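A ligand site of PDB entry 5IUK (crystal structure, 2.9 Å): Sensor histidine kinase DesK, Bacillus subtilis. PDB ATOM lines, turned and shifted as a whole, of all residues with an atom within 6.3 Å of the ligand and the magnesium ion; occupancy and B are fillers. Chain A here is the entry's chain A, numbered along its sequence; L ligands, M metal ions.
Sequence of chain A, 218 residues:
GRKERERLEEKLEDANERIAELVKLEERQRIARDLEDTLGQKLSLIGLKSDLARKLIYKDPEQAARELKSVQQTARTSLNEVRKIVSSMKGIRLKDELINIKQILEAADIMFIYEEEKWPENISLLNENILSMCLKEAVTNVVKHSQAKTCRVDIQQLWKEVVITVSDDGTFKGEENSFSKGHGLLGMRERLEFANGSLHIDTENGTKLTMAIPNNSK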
ATOM      1  N   GLU A 137     -22.371   0.644  36.770  1.00  0.00           N
ATOM      2  CA  GLU A 137     -23.377   0.640  35.731  1.00  0.00           C
ATOM      3  C   GLU A 137     -22.891   0.026  34.395  1.00  0.00           C
ATOM      4  O   GLU A 137     -23.632  -0.709  33.738  1.00  0.00           O
ATOM      5  CB  GLU A 137     -23.957   2.048  35.537  1.00  0.00           C
ATOM      6  CG  GLU A 137     -24.931   2.169  34.373  1.00  0.00           C
ATOM      7  CD  GLU A 137     -26.157   1.254  34.309  1.00  0.00           C
ATOM      8  OE1 GLU A 137     -26.509   0.612  35.330  1.00  0.00           O
ATOM      9  OE2 GLU A 137     -26.794   1.232  33.239  1.00  0.00           O
ATOM     10  N   ALA A 138     -21.645   0.343  33.999  1.00  0.00           N
ATOM     11  CA  ALA A 138     -21.040  -0.166  32.774  1.00  0.00           C
ATOM     12  C   ALA A 138     -21.073  -1.694  32.834  1.00  0.00           C
ATOM     13  O   ALA A 138     -21.514  -2.332  31.877  1.00  0.00           O
ATOM     14  CB  ALA A 138     -19.617   0.338  32.631  1.00  0.00           C
ATOM     15  N   THR A 140     -22.976  -3.640  35.004  1.00  0.00           N
ATOM     16  CA  THR A 140     -24.374  -4.093  35.081  1.00  0.00           C
ATOM     17  C   THR A 140     -24.906  -4.254  33.657  1.00  0.00           C
ATOM     18  O   THR A 140     -25.574  -5.244  33.355  1.00  0.00           O
ATOM     19  CB  THR A 140     -25.215  -3.084  35.849  1.00  0.00           C
ATOM     20  OG1 THR A 140     -24.718  -2.987  37.177  1.00  0.00           O
ATOM     21  CG2 THR A 140     -26.710  -3.441  35.863  1.00  0.00           C
ATOM     22  N   ASN A 141     -24.568  -3.305  32.763  1.00  0.00           N
ATOM     23  CA  ASN A 141     -25.011  -3.354  31.383  1.00  0.00           C
ATOM     24  C   ASN A 141     -24.405  -4.534  30.636  1.00  0.00           C
ATOM     25  O   ASN A 141     -25.092  -5.171  29.836  1.00  0.00           O
ATOM     26  CB  ASN A 141     -24.704  -2.060  30.649  1.00  0.00           C
ATOM     27  CG  ASN A 141     -25.666  -0.942  30.946  1.00  0.00           C
ATOM     28  OD1 ASN A 141     -26.773  -1.134  31.489  1.00  0.00           O
ATOM     29  ND2 ASN A 141     -25.267   0.270  30.567  1.00  0.00           N
ATOM     30  N   VAL A 142     -23.122  -4.810  30.878  1.00  0.00           N
ATOM     31  CA  VAL A 142     -22.453  -5.946  30.267  1.00  0.00           C
ATOM     32  C   VAL A 142     -23.218  -7.209  30.658  1.00  0.00           C
ATOM     33  O   VAL A 142     -23.613  -7.991  29.794  1.00  0.00           O
ATOM     34  CB  VAL A 142     -20.955  -6.032  30.695  1.00  0.00           C
ATOM     35  CG1 VAL A 142     -20.338  -7.368  30.274  1.00  0.00           C
ATOM     36  CG2 VAL A 142     -20.148  -4.882  30.117  1.00  0.00           C
ATOM     37  N   VAL A 143     -23.454  -7.391  31.967  1.00  0.00           N
ATOM     38  CA  VAL A 143     -24.105  -8.594  32.485  1.00  0.00           C
ATOM     39  C   VAL A 143     -25.552  -8.781  31.945  1.00  0.00           C
ATOM     40  O   VAL A 143     -25.916  -9.881  31.523  1.00  0.00           O
ATOM     41  CB  VAL A 143     -24.031  -8.662  34.053  1.00  0.00           C
ATOM     42  CG1 VAL A 143     -24.873  -9.799  34.614  1.00  0.00           C
ATOM     43  CG2 VAL A 143     -22.576  -8.745  34.553  1.00  0.00           C
ATOM     44  N   LYS A 144     -26.343  -7.713  31.963  1.00  0.00           N
ATOM     45  CA  LYS A 144     -27.748  -7.749  31.590  1.00  0.00           C
ATOM     46  C   LYS A 144     -28.011  -7.864  30.114  1.00  0.00           C
ATOM     47  O   LYS A 144     -29.037  -8.421  29.736  1.00  0.00           O
ATOM     48  CB  LYS A 144     -28.465  -6.464  32.054  1.00  0.00           C
ATOM     49  CG  LYS A 144     -28.547  -6.215  33.548  1.00  0.00           C
ATOM     50  CD  LYS A 144     -29.725  -5.313  33.931  1.00  0.00           C
ATOM     51  CE  LYS A 144     -29.777  -3.949  33.271  1.00  0.00           C
ATOM     52  NZ  LYS A 144     -30.849  -3.126  33.893  1.00  0.00           N
ATOM     53  N   HIS A 145     -27.156  -7.240  29.281  1.00  0.00           N
ATOM     54  CA  HIS A 145     -27.456  -7.114  27.853  1.00  0.00           C
ATOM     55  C   HIS A 145     -26.508  -7.697  26.818  1.00  0.00           C
ATOM     56  O   HIS A 145     -26.962  -8.035  25.723  1.00  0.00           O
ATOM     57  CB  HIS A 145     -27.604  -5.620  27.483  1.00  0.00           C
ATOM     58  CG  HIS A 145     -28.413  -4.756  28.416  1.00  0.00           C
ATOM     59  ND1 HIS A 145     -29.790  -4.910  28.526  1.00  0.00           N
ATOM     60  CD2 HIS A 145     -28.039  -3.697  29.168  1.00  0.00           C
ATOM     61  CE1 HIS A 145     -30.183  -3.975  29.372  1.00  0.00           C
ATOM     62  NE2 HIS A 145     -29.160  -3.236  29.796  1.00  0.00           N
ATOM     63  N   SER A 146     -25.206  -7.704  27.091  1.00  0.00           N
ATOM     64  CA  SER A 146     -24.216  -7.982  26.062  1.00  0.00           C
ATOM     65  C   SER A 146     -24.175  -9.386  25.473  1.00  0.00           C
ATOM     66  O   SER A 146     -23.911  -9.521  24.278  1.00  0.00           O
ATOM     67  CB  SER A 146     -22.817  -7.616  26.559  1.00  0.00           C
ATOM     68  OG  SER A 146     -22.349  -8.547  27.516  1.00  0.00           O
ATOM     69  N   GLN A 147     -24.389 -10.413  26.306  1.00  0.00           N
ATOM     70  CA  GLN A 147     -24.163 -11.836  26.003  1.00  0.00           C
ATOM     71  C   GLN A 147     -22.640 -12.061  25.750  1.00  0.00           C
ATOM     72  O   GLN A 147     -22.245 -12.970  25.017  1.00  0.00           O
ATOM     73  CB  GLN A 147     -25.007 -12.355  24.825  1.00  0.00           C
ATOM     74  CG  GLN A 147     -26.504 -12.225  24.994  1.00  0.00           C
ATOM     75  CD  GLN A 147     -27.159 -12.411  23.654  1.00  0.00           C
ATOM     76  OE1 GLN A 147     -26.946 -11.626  22.728  1.00  0.00           O
ATOM     77  NE2 GLN A 147     -27.922 -13.479  23.483  1.00  0.00           N
ATOM     78  N   ASP A 168     -16.499  -5.043  26.149  1.00  0.00           N
ATOM     79  CA  ASP A 168     -17.013  -6.405  26.147  1.00  0.00           C
ATOM     80  C   ASP A 168     -17.097  -6.898  24.712  1.00  0.00           C
ATOM     81  O   ASP A 168     -17.165  -6.092  23.768  1.00  0.00           O
ATOM     82  CB  ASP A 168     -18.326  -6.533  26.930  1.00  0.00           C
ATOM     83  CG  ASP A 168     -19.536  -6.008  26.195  1.00  0.00           C
ATOM     84  OD1 ASP A 168     -19.916  -6.609  25.168  1.00  0.00           O
ATOM     85  OD2 ASP A 168     -20.130  -5.013  26.654  1.00  0.00           O
ATOM     86  N   GLY A 170     -19.530  -8.891  23.466  1.00  0.00           N
ATOM     87  CA  GLY A 170     -20.886  -9.286  23.125  1.00  0.00           C
ATOM     88  C   GLY A 170     -21.391  -8.478  21.944  1.00  0.00           C
ATOM     89  O   GLY A 170     -20.612  -8.065  21.077  1.00  0.00           O
ATOM     90  N   THR A 171     -22.713  -8.272  21.865  1.00  0.00           N
ATOM     91  CA  THR A 171     -23.297  -7.450  20.805  1.00  0.00           C
ATOM     92  C   THR A 171     -24.147  -6.358  21.419  1.00  0.00           C
ATOM     93  O   THR A 171     -24.913  -6.610  22.363  1.00  0.00           O
ATOM     94  CB  THR A 171     -24.074  -8.255  19.744  1.00  0.00           C
ATOM     95  OG1 THR A 171     -25.138  -8.977  20.349  1.00  0.00           O
ATOM     96  CG2 THR A 171     -23.181  -9.183  18.939  1.00  0.00           C
ATOM     97  N   PHE A 172     -23.988  -5.141  20.901  1.00  0.00           N
ATOM     98  CA  PHE A 172     -24.751  -3.993  21.365  1.00  0.00           C
ATOM     99  C   PHE A 172     -26.223  -4.138  20.988  1.00  0.00           C
ATOM    100  O   PHE A 172     -26.544  -4.484  19.848  1.00  0.00           O
ATOM    101  CB  PHE A 172     -24.142  -2.689  20.882  1.00  0.00           C
ATOM    102  CG  PHE A 172     -24.751  -1.485  21.549  1.00  0.00           C
ATOM    103  CD1 PHE A 172     -24.449  -1.170  22.862  1.00  0.00           C
ATOM    104  CD2 PHE A 172     -25.656  -0.686  20.873  1.00  0.00           C
ATOM    105  CE1 PHE A 172     -25.035  -0.077  23.485  1.00  0.00           C
ATOM    106  CE2 PHE A 172     -26.236   0.417  21.488  1.00  0.00           C
ATOM    107  CZ  PHE A 172     -25.934   0.715  22.805  1.00  0.00           C
ATOM    108  N   LYS A 173     -27.111  -3.908  21.953  1.00  0.00           N
ATOM    109  CA  LYS A 173     -28.539  -4.133  21.788  1.00  0.00           C
ATOM    110  C   LYS A 173     -29.384  -2.889  21.570  1.00  0.00           C
ATOM    111  O   LYS A 173     -30.576  -3.005  21.243  1.00  0.00           O
ATOM    112  CB  LYS A 173     -29.084  -4.958  22.981  1.00  0.00           C
ATOM    113  CG  LYS A 173     -28.398  -6.292  23.231  1.00  0.00           C
ATOM    114  CD  LYS A 173     -28.368  -7.218  22.014  1.00  0.00           C
ATOM    115  CE  LYS A 173     -28.024  -8.640  22.400  1.00  0.00           C
ATOM    116  NZ  LYS A 173     -26.673  -8.723  23.033  1.00  0.00           N
ATOM    117  N   GLY A 174     -28.789  -1.720  21.735  1.00  0.00           N
ATOM    118  CA  GLY A 174     -29.518  -0.463  21.590  1.00  0.00           C
ATOM    119  C   GLY A 174     -29.713   0.034  20.166  1.00  0.00           C
ATOM    120  O   GLY A 174     -29.116  -0.490  19.209  1.00  0.00           O
ATOM    121  N   GLU A 175     -30.535   1.083  20.026  1.00  0.00           N
ATOM    122  CA  GLU A 175     -30.789   1.749  18.751  1.00  0.00           C
ATOM    123  C   GLU A 175     -29.612   2.674  18.426  1.00  0.00           C
ATOM    124  O   GLU A 175     -28.707   2.833  19.246  1.00  0.00           O
ATOM    125  CB  GLU A 175     -32.098   2.554  18.827  1.00  0.00           C
ATOM    126  N   HIS A 183     -32.266   6.503  32.104  1.00  0.00           N
ATOM    127  CA  HIS A 183     -31.499   5.253  32.071  1.00  0.00           C
ATOM    128  C   HIS A 183     -30.004   5.469  32.370  1.00  0.00           C
ATOM    129  O   HIS A 183     -29.566   6.614  32.516  1.00  0.00           O
ATOM    130  CB  HIS A 183     -31.726   4.515  30.743  1.00  0.00           C
ATOM    131  CG  HIS A 183     -33.140   4.094  30.522  1.00  0.00           C
ATOM    132  ND1 HIS A 183     -33.731   3.099  31.293  1.00  0.00           N
ATOM    133  CD2 HIS A 183     -34.037   4.532  29.619  1.00  0.00           C
ATOM    134  CE1 HIS A 183     -34.956   2.980  30.828  1.00  0.00           C
ATOM    135  NE2 HIS A 183     -35.192   3.810  29.822  1.00  0.00           N
ATOM    136  N   GLY A 184     -29.256   4.370  32.476  1.00  0.00           N
ATOM    137  CA  GLY A 184     -27.839   4.359  32.826  1.00  0.00           C
ATOM    138  C   GLY A 184     -26.851   5.027  31.891  1.00  0.00           C
ATOM    139  O   GLY A 184     -25.899   5.659  32.370  1.00  0.00           O
ATOM    140  N   LEU A 185     -27.037   4.905  30.558  1.00  0.00           N
ATOM    141  CA  LEU A 185     -26.099   5.523  29.618  1.00  0.00           C
ATOM    142  C   LEU A 185     -26.128   7.060  29.706  1.00  0.00           C
ATOM    143  O   LEU A 185     -25.066   7.693  29.822  1.00  0.00           O
ATOM    144  CB  LEU A 185     -26.268   4.991  28.203  1.00  0.00           C
ATOM    145  CG  LEU A 185     -25.648   3.594  28.004  1.00  0.00           C
ATOM    146  CD1 LEU A 185     -26.189   2.898  26.781  1.00  0.00           C
ATOM    147  CD2 LEU A 185     -24.141   3.642  27.989  1.00  0.00           C
ATOM    148  N   LEU A 186     -27.323   7.637  29.760  1.00  0.00           N
ATOM    149  CA  LEU A 186     -27.458   9.077  29.975  1.00  0.00           C
ATOM    150  C   LEU A 186     -27.053   9.468  31.403  1.00  0.00           C
ATOM    151  O   LEU A 186     -26.440  10.514  31.600  1.00  0.00           O
ATOM    152  CB  LEU A 186     -28.883   9.539  29.654  1.00  0.00           C
ATOM    153  CG  LEU A 186     -29.113  11.041  29.710  1.00  0.00           C
ATOM    154  CD1 LEU A 186     -28.134  11.802  28.797  1.00  0.00           C
ATOM    155  CD2 LEU A 186     -30.540  11.358  29.429  1.00  0.00           C
ATOM    156  N   MET A 188     -24.758   8.005  33.399  1.00  0.00           N
ATOM    157  CA  MET A 188     -23.305   8.039  33.428  1.00  0.00           C
ATOM    158  C   MET A 188     -22.769   9.283  32.715  1.00  0.00           C
ATOM    159  O   MET A 188     -21.906   9.979  33.249  1.00  0.00           O
ATOM    160  CB  MET A 188     -22.724   6.808  32.724  1.00  0.00           C
ATOM    161  CG  MET A 188     -22.840   5.542  33.513  1.00  0.00           C
ATOM    162  SD  MET A 188     -21.905   4.252  32.651  1.00  0.00           S
ATOM    163  CE  MET A 188     -23.006   3.885  31.461  1.00  0.00           C
ATOM    164  N   ILE A 201     -18.692   6.123  23.535  1.00  0.00           N
ATOM    165  CA  ILE A 201     -19.104   4.752  23.304  1.00  0.00           C
ATOM    166  C   ILE A 201     -18.768   4.337  21.863  1.00  0.00           C
ATOM    167  O   ILE A 201     -18.916   5.114  20.932  1.00  0.00           O
ATOM    168  CB  ILE A 201     -20.606   4.554  23.673  1.00  0.00           C
ATOM    169  CG1 ILE A 201     -21.026   3.056  23.662  1.00  0.00           C
ATOM    170  CG2 ILE A 201     -21.525   5.411  22.788  1.00  0.00           C
ATOM    171  CD1 ILE A 201     -22.382   2.742  24.285  1.00  0.00           C
ATOM    172  N   THR A 207     -19.180  -3.703  22.757  1.00  0.00           N
ATOM    173  CA  THR A 207     -19.449  -2.378  23.303  1.00  0.00           C
ATOM    174  C   THR A 207     -18.272  -1.934  24.129  1.00  0.00           C
ATOM    175  O   THR A 207     -17.815  -2.669  25.017  1.00  0.00           O
ATOM    176  CB  THR A 207     -20.711  -2.414  24.200  1.00  0.00           C
ATOM    177  OG1 THR A 207     -21.803  -2.988  23.473  1.00  0.00           O
ATOM    178  CG2 THR A 207     -21.072  -1.037  24.775  1.00  0.00           C
HETATM  179  P1  LIG L   1     -31.094   0.759  33.618  1.00  0.00           P
HETATM  180  O1  LIG L   1     -31.748   1.939  34.267  1.00  0.00           O
HETATM  181  O2  LIG L   1     -31.072  -0.478  34.547  1.00  0.00           O
HETATM  182  O3  LIG L   1     -29.626   1.033  33.226  1.00  0.00           O
HETATM  183  P2  LIG L   1     -31.040  -0.057  30.651  1.00  0.00           P
HETATM  184  O4  LIG L   1     -31.765  -0.780  29.529  1.00  0.00           O
HETATM  185  O5  LIG L   1     -29.861  -0.943  31.158  1.00  0.00           O
HETATM  186  C1  LIG L   1     -31.992   0.304  32.134  1.00  0.00           C
HETATM  187  P3  LIG L   1     -29.018   1.766  29.524  1.00  0.00           P
HETATM  188  O6  LIG L   1     -27.910   1.350  30.405  1.00  0.00           O
HETATM  189  O7  LIG L   1     -29.017   3.289  29.370  1.00  0.00           O
HETATM  190  O8  LIG L   1     -30.422   1.351  30.153  1.00  0.00           O
HETATM  191  O9  LIG L   1     -28.848   1.108  28.074  1.00  0.00           O
HETATM  192  C2  LIG L   1     -29.837   1.326  27.047  1.00  0.00           C
HETATM  193  C3  LIG L   1     -29.830   0.174  26.090  1.00  0.00           C
HETATM  194  O10 LIG L   1     -28.533   0.041  25.483  1.00  0.00           O
HETATM  195  C4  LIG L   1     -30.142  -1.192  26.693  1.00  0.00           C
HETATM  196  O11 LIG L   1     -31.544  -1.411  26.783  1.00  0.00           O
HETATM  197  C5  LIG L   1     -29.451  -2.146  25.712  1.00  0.00           C
HETATM  198  O12 LIG L   1     -30.283  -2.455  24.600  1.00  0.00           O
HETATM  199  C6  LIG L   1     -28.223  -1.332  25.288  1.00  0.00           C
HETATM  200  N1  LIG L   1     -26.986  -1.647  26.003  1.00  0.00           N
HETATM  201  C7  LIG L   1     -26.405  -0.896  27.000  1.00  0.00           C
HETATM  202  N2  LIG L   1     -25.269  -1.382  27.445  1.00  0.00           N
HETATM  203  C8  LIG L   1     -25.091  -2.532  26.686  1.00  0.00           C
HETATM  204  C9  LIG L   1     -24.059  -3.503  26.658  1.00  0.00           C
HETATM  205  N3  LIG L   1     -23.002  -3.492  27.469  1.00  0.00           N
HETATM  206  N4  LIG L   1     -24.164  -4.512  25.764  1.00  0.00           N
HETATM  207  C10 LIG L   1     -25.242  -4.546  24.962  1.00  0.00           C
HETATM  208  N5  LIG L   1     -26.271  -3.706  24.909  1.00  0.00           N
HETATM  209  C11 LIG L   1     -26.145  -2.709  25.802  1.00  0.00           C
HETATM  210 MG    MG M   1     -28.229   0.047  32.307  1.00  0.00          MG
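N of Asp 168 is in hydrogen-bond range of O of Thr 207 (2.9 Å).
The backbone carbonyl oxygen (O) of Val 142 sits at hydrogen-bond distance from the side-chain hydroxyl (OG) of Ser 146, 2.7 Å away.
The backbone NH (N) of Thr 171 is in hydrogen-bond range of the backbone carbonyl oxygen (O) of Ser 146 (3.0 Å).
The side-chain carboxylate (OD1) of Asp 168 is in hydrogen-bond range of the backbone NH (N) of Gly 170 (2.9 Å).
O of His 145 lies within hydrogen-bond range of NZ of Lys 173, 2.8 Å away.
O of Ser 146 is in hydrogen-bond range of NZ of Lys 173.
The side-chain amino group (NZ) of Lys 173 is in hydrogen-bond range of the backbone carbonyl oxygen (O) of Thr 171, 2.8 Å away.
OE1 of Gln 147 is in hydrogen-bond range of NZ of Lys 173 (2.9 Å).
The magnesium ion is bound by an oxygen (O3) of the ligand (1.9 Å), the side-chain amide oxygen (OD1) of Asn 141 (2.0 Å), the side-chain carboxylate (OE2) of Glu 137 (2.1 Å), an oxygen (O5) of the ligand (2.2 Å) and an oxygen (O6) of the ligand (2.3 Å).
The side-chain amino group (NZ) of Lys 144 lies within salt-bridge range of an oxygen (O2) of the ligand (2.7 Å).
A ring nitrogen (NE2) of His 145 lies close to an oxygen (O5) of the ligand (2.8 Å).
O12 of the ligand sits close to O of Lys 173 (3.4 Å).
The backbone NH (N) of Leu 185 lies within hydrogen-bond range of an oxygen (O7) of the ligand, 2.8 Å away.
An oxygen (O12) of the ligand lies within hydrogen-bond range of the backbone NH (N) of Gly 174 (3.3 Å).
A nitrogen (N3) of the ligand lies within hydrogen-bond range of the side-chain carboxylate of Asp 168 (3.4 Å).
The backbone NH (N) of Lys 173 lies within hydrogen-bond range of a nitrogen (N5) of the ligand (3.1 Å).
N of Gly 184 is in hydrogen-bond range of O7 of the ligand (3.3 Å).
Within 4 Å of the magnesium ion: Glu 137 and Asn 141.
The nearest printed residue that does not touch the magnesium ion is His 145 (4.2 Å).
Val 142 touches the ligand (N to N3, 3.7 Å).
Ser 146 touches the ligand.
Thr 171 touches the ligand (O to C10, 3.3 Å).
CE1 of Phe 172 touches N1 of the ligand (3.6 Å).
His 183 touches the ligand.
Thr 207 touches the ligand.
Hydrophobic or aromatic side chains that line the ligand: His 145, Phe 172, His 183 and Leu 185.
Within 4 Å of the ligand: Glu 137, Asn 141, Val 142, Lys 144, His 145, Ser 146, Asp 168, Thr 171, Phe 172, Lys 173, Gly 174, His 183, Gly 184, Leu 185 and Thr 207.
Along chain A the residues within 4 Å of the ligand span positions 137 to 207.
The nearest printed residue that does not touch the ligand is Leu 186 (4.7 Å).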
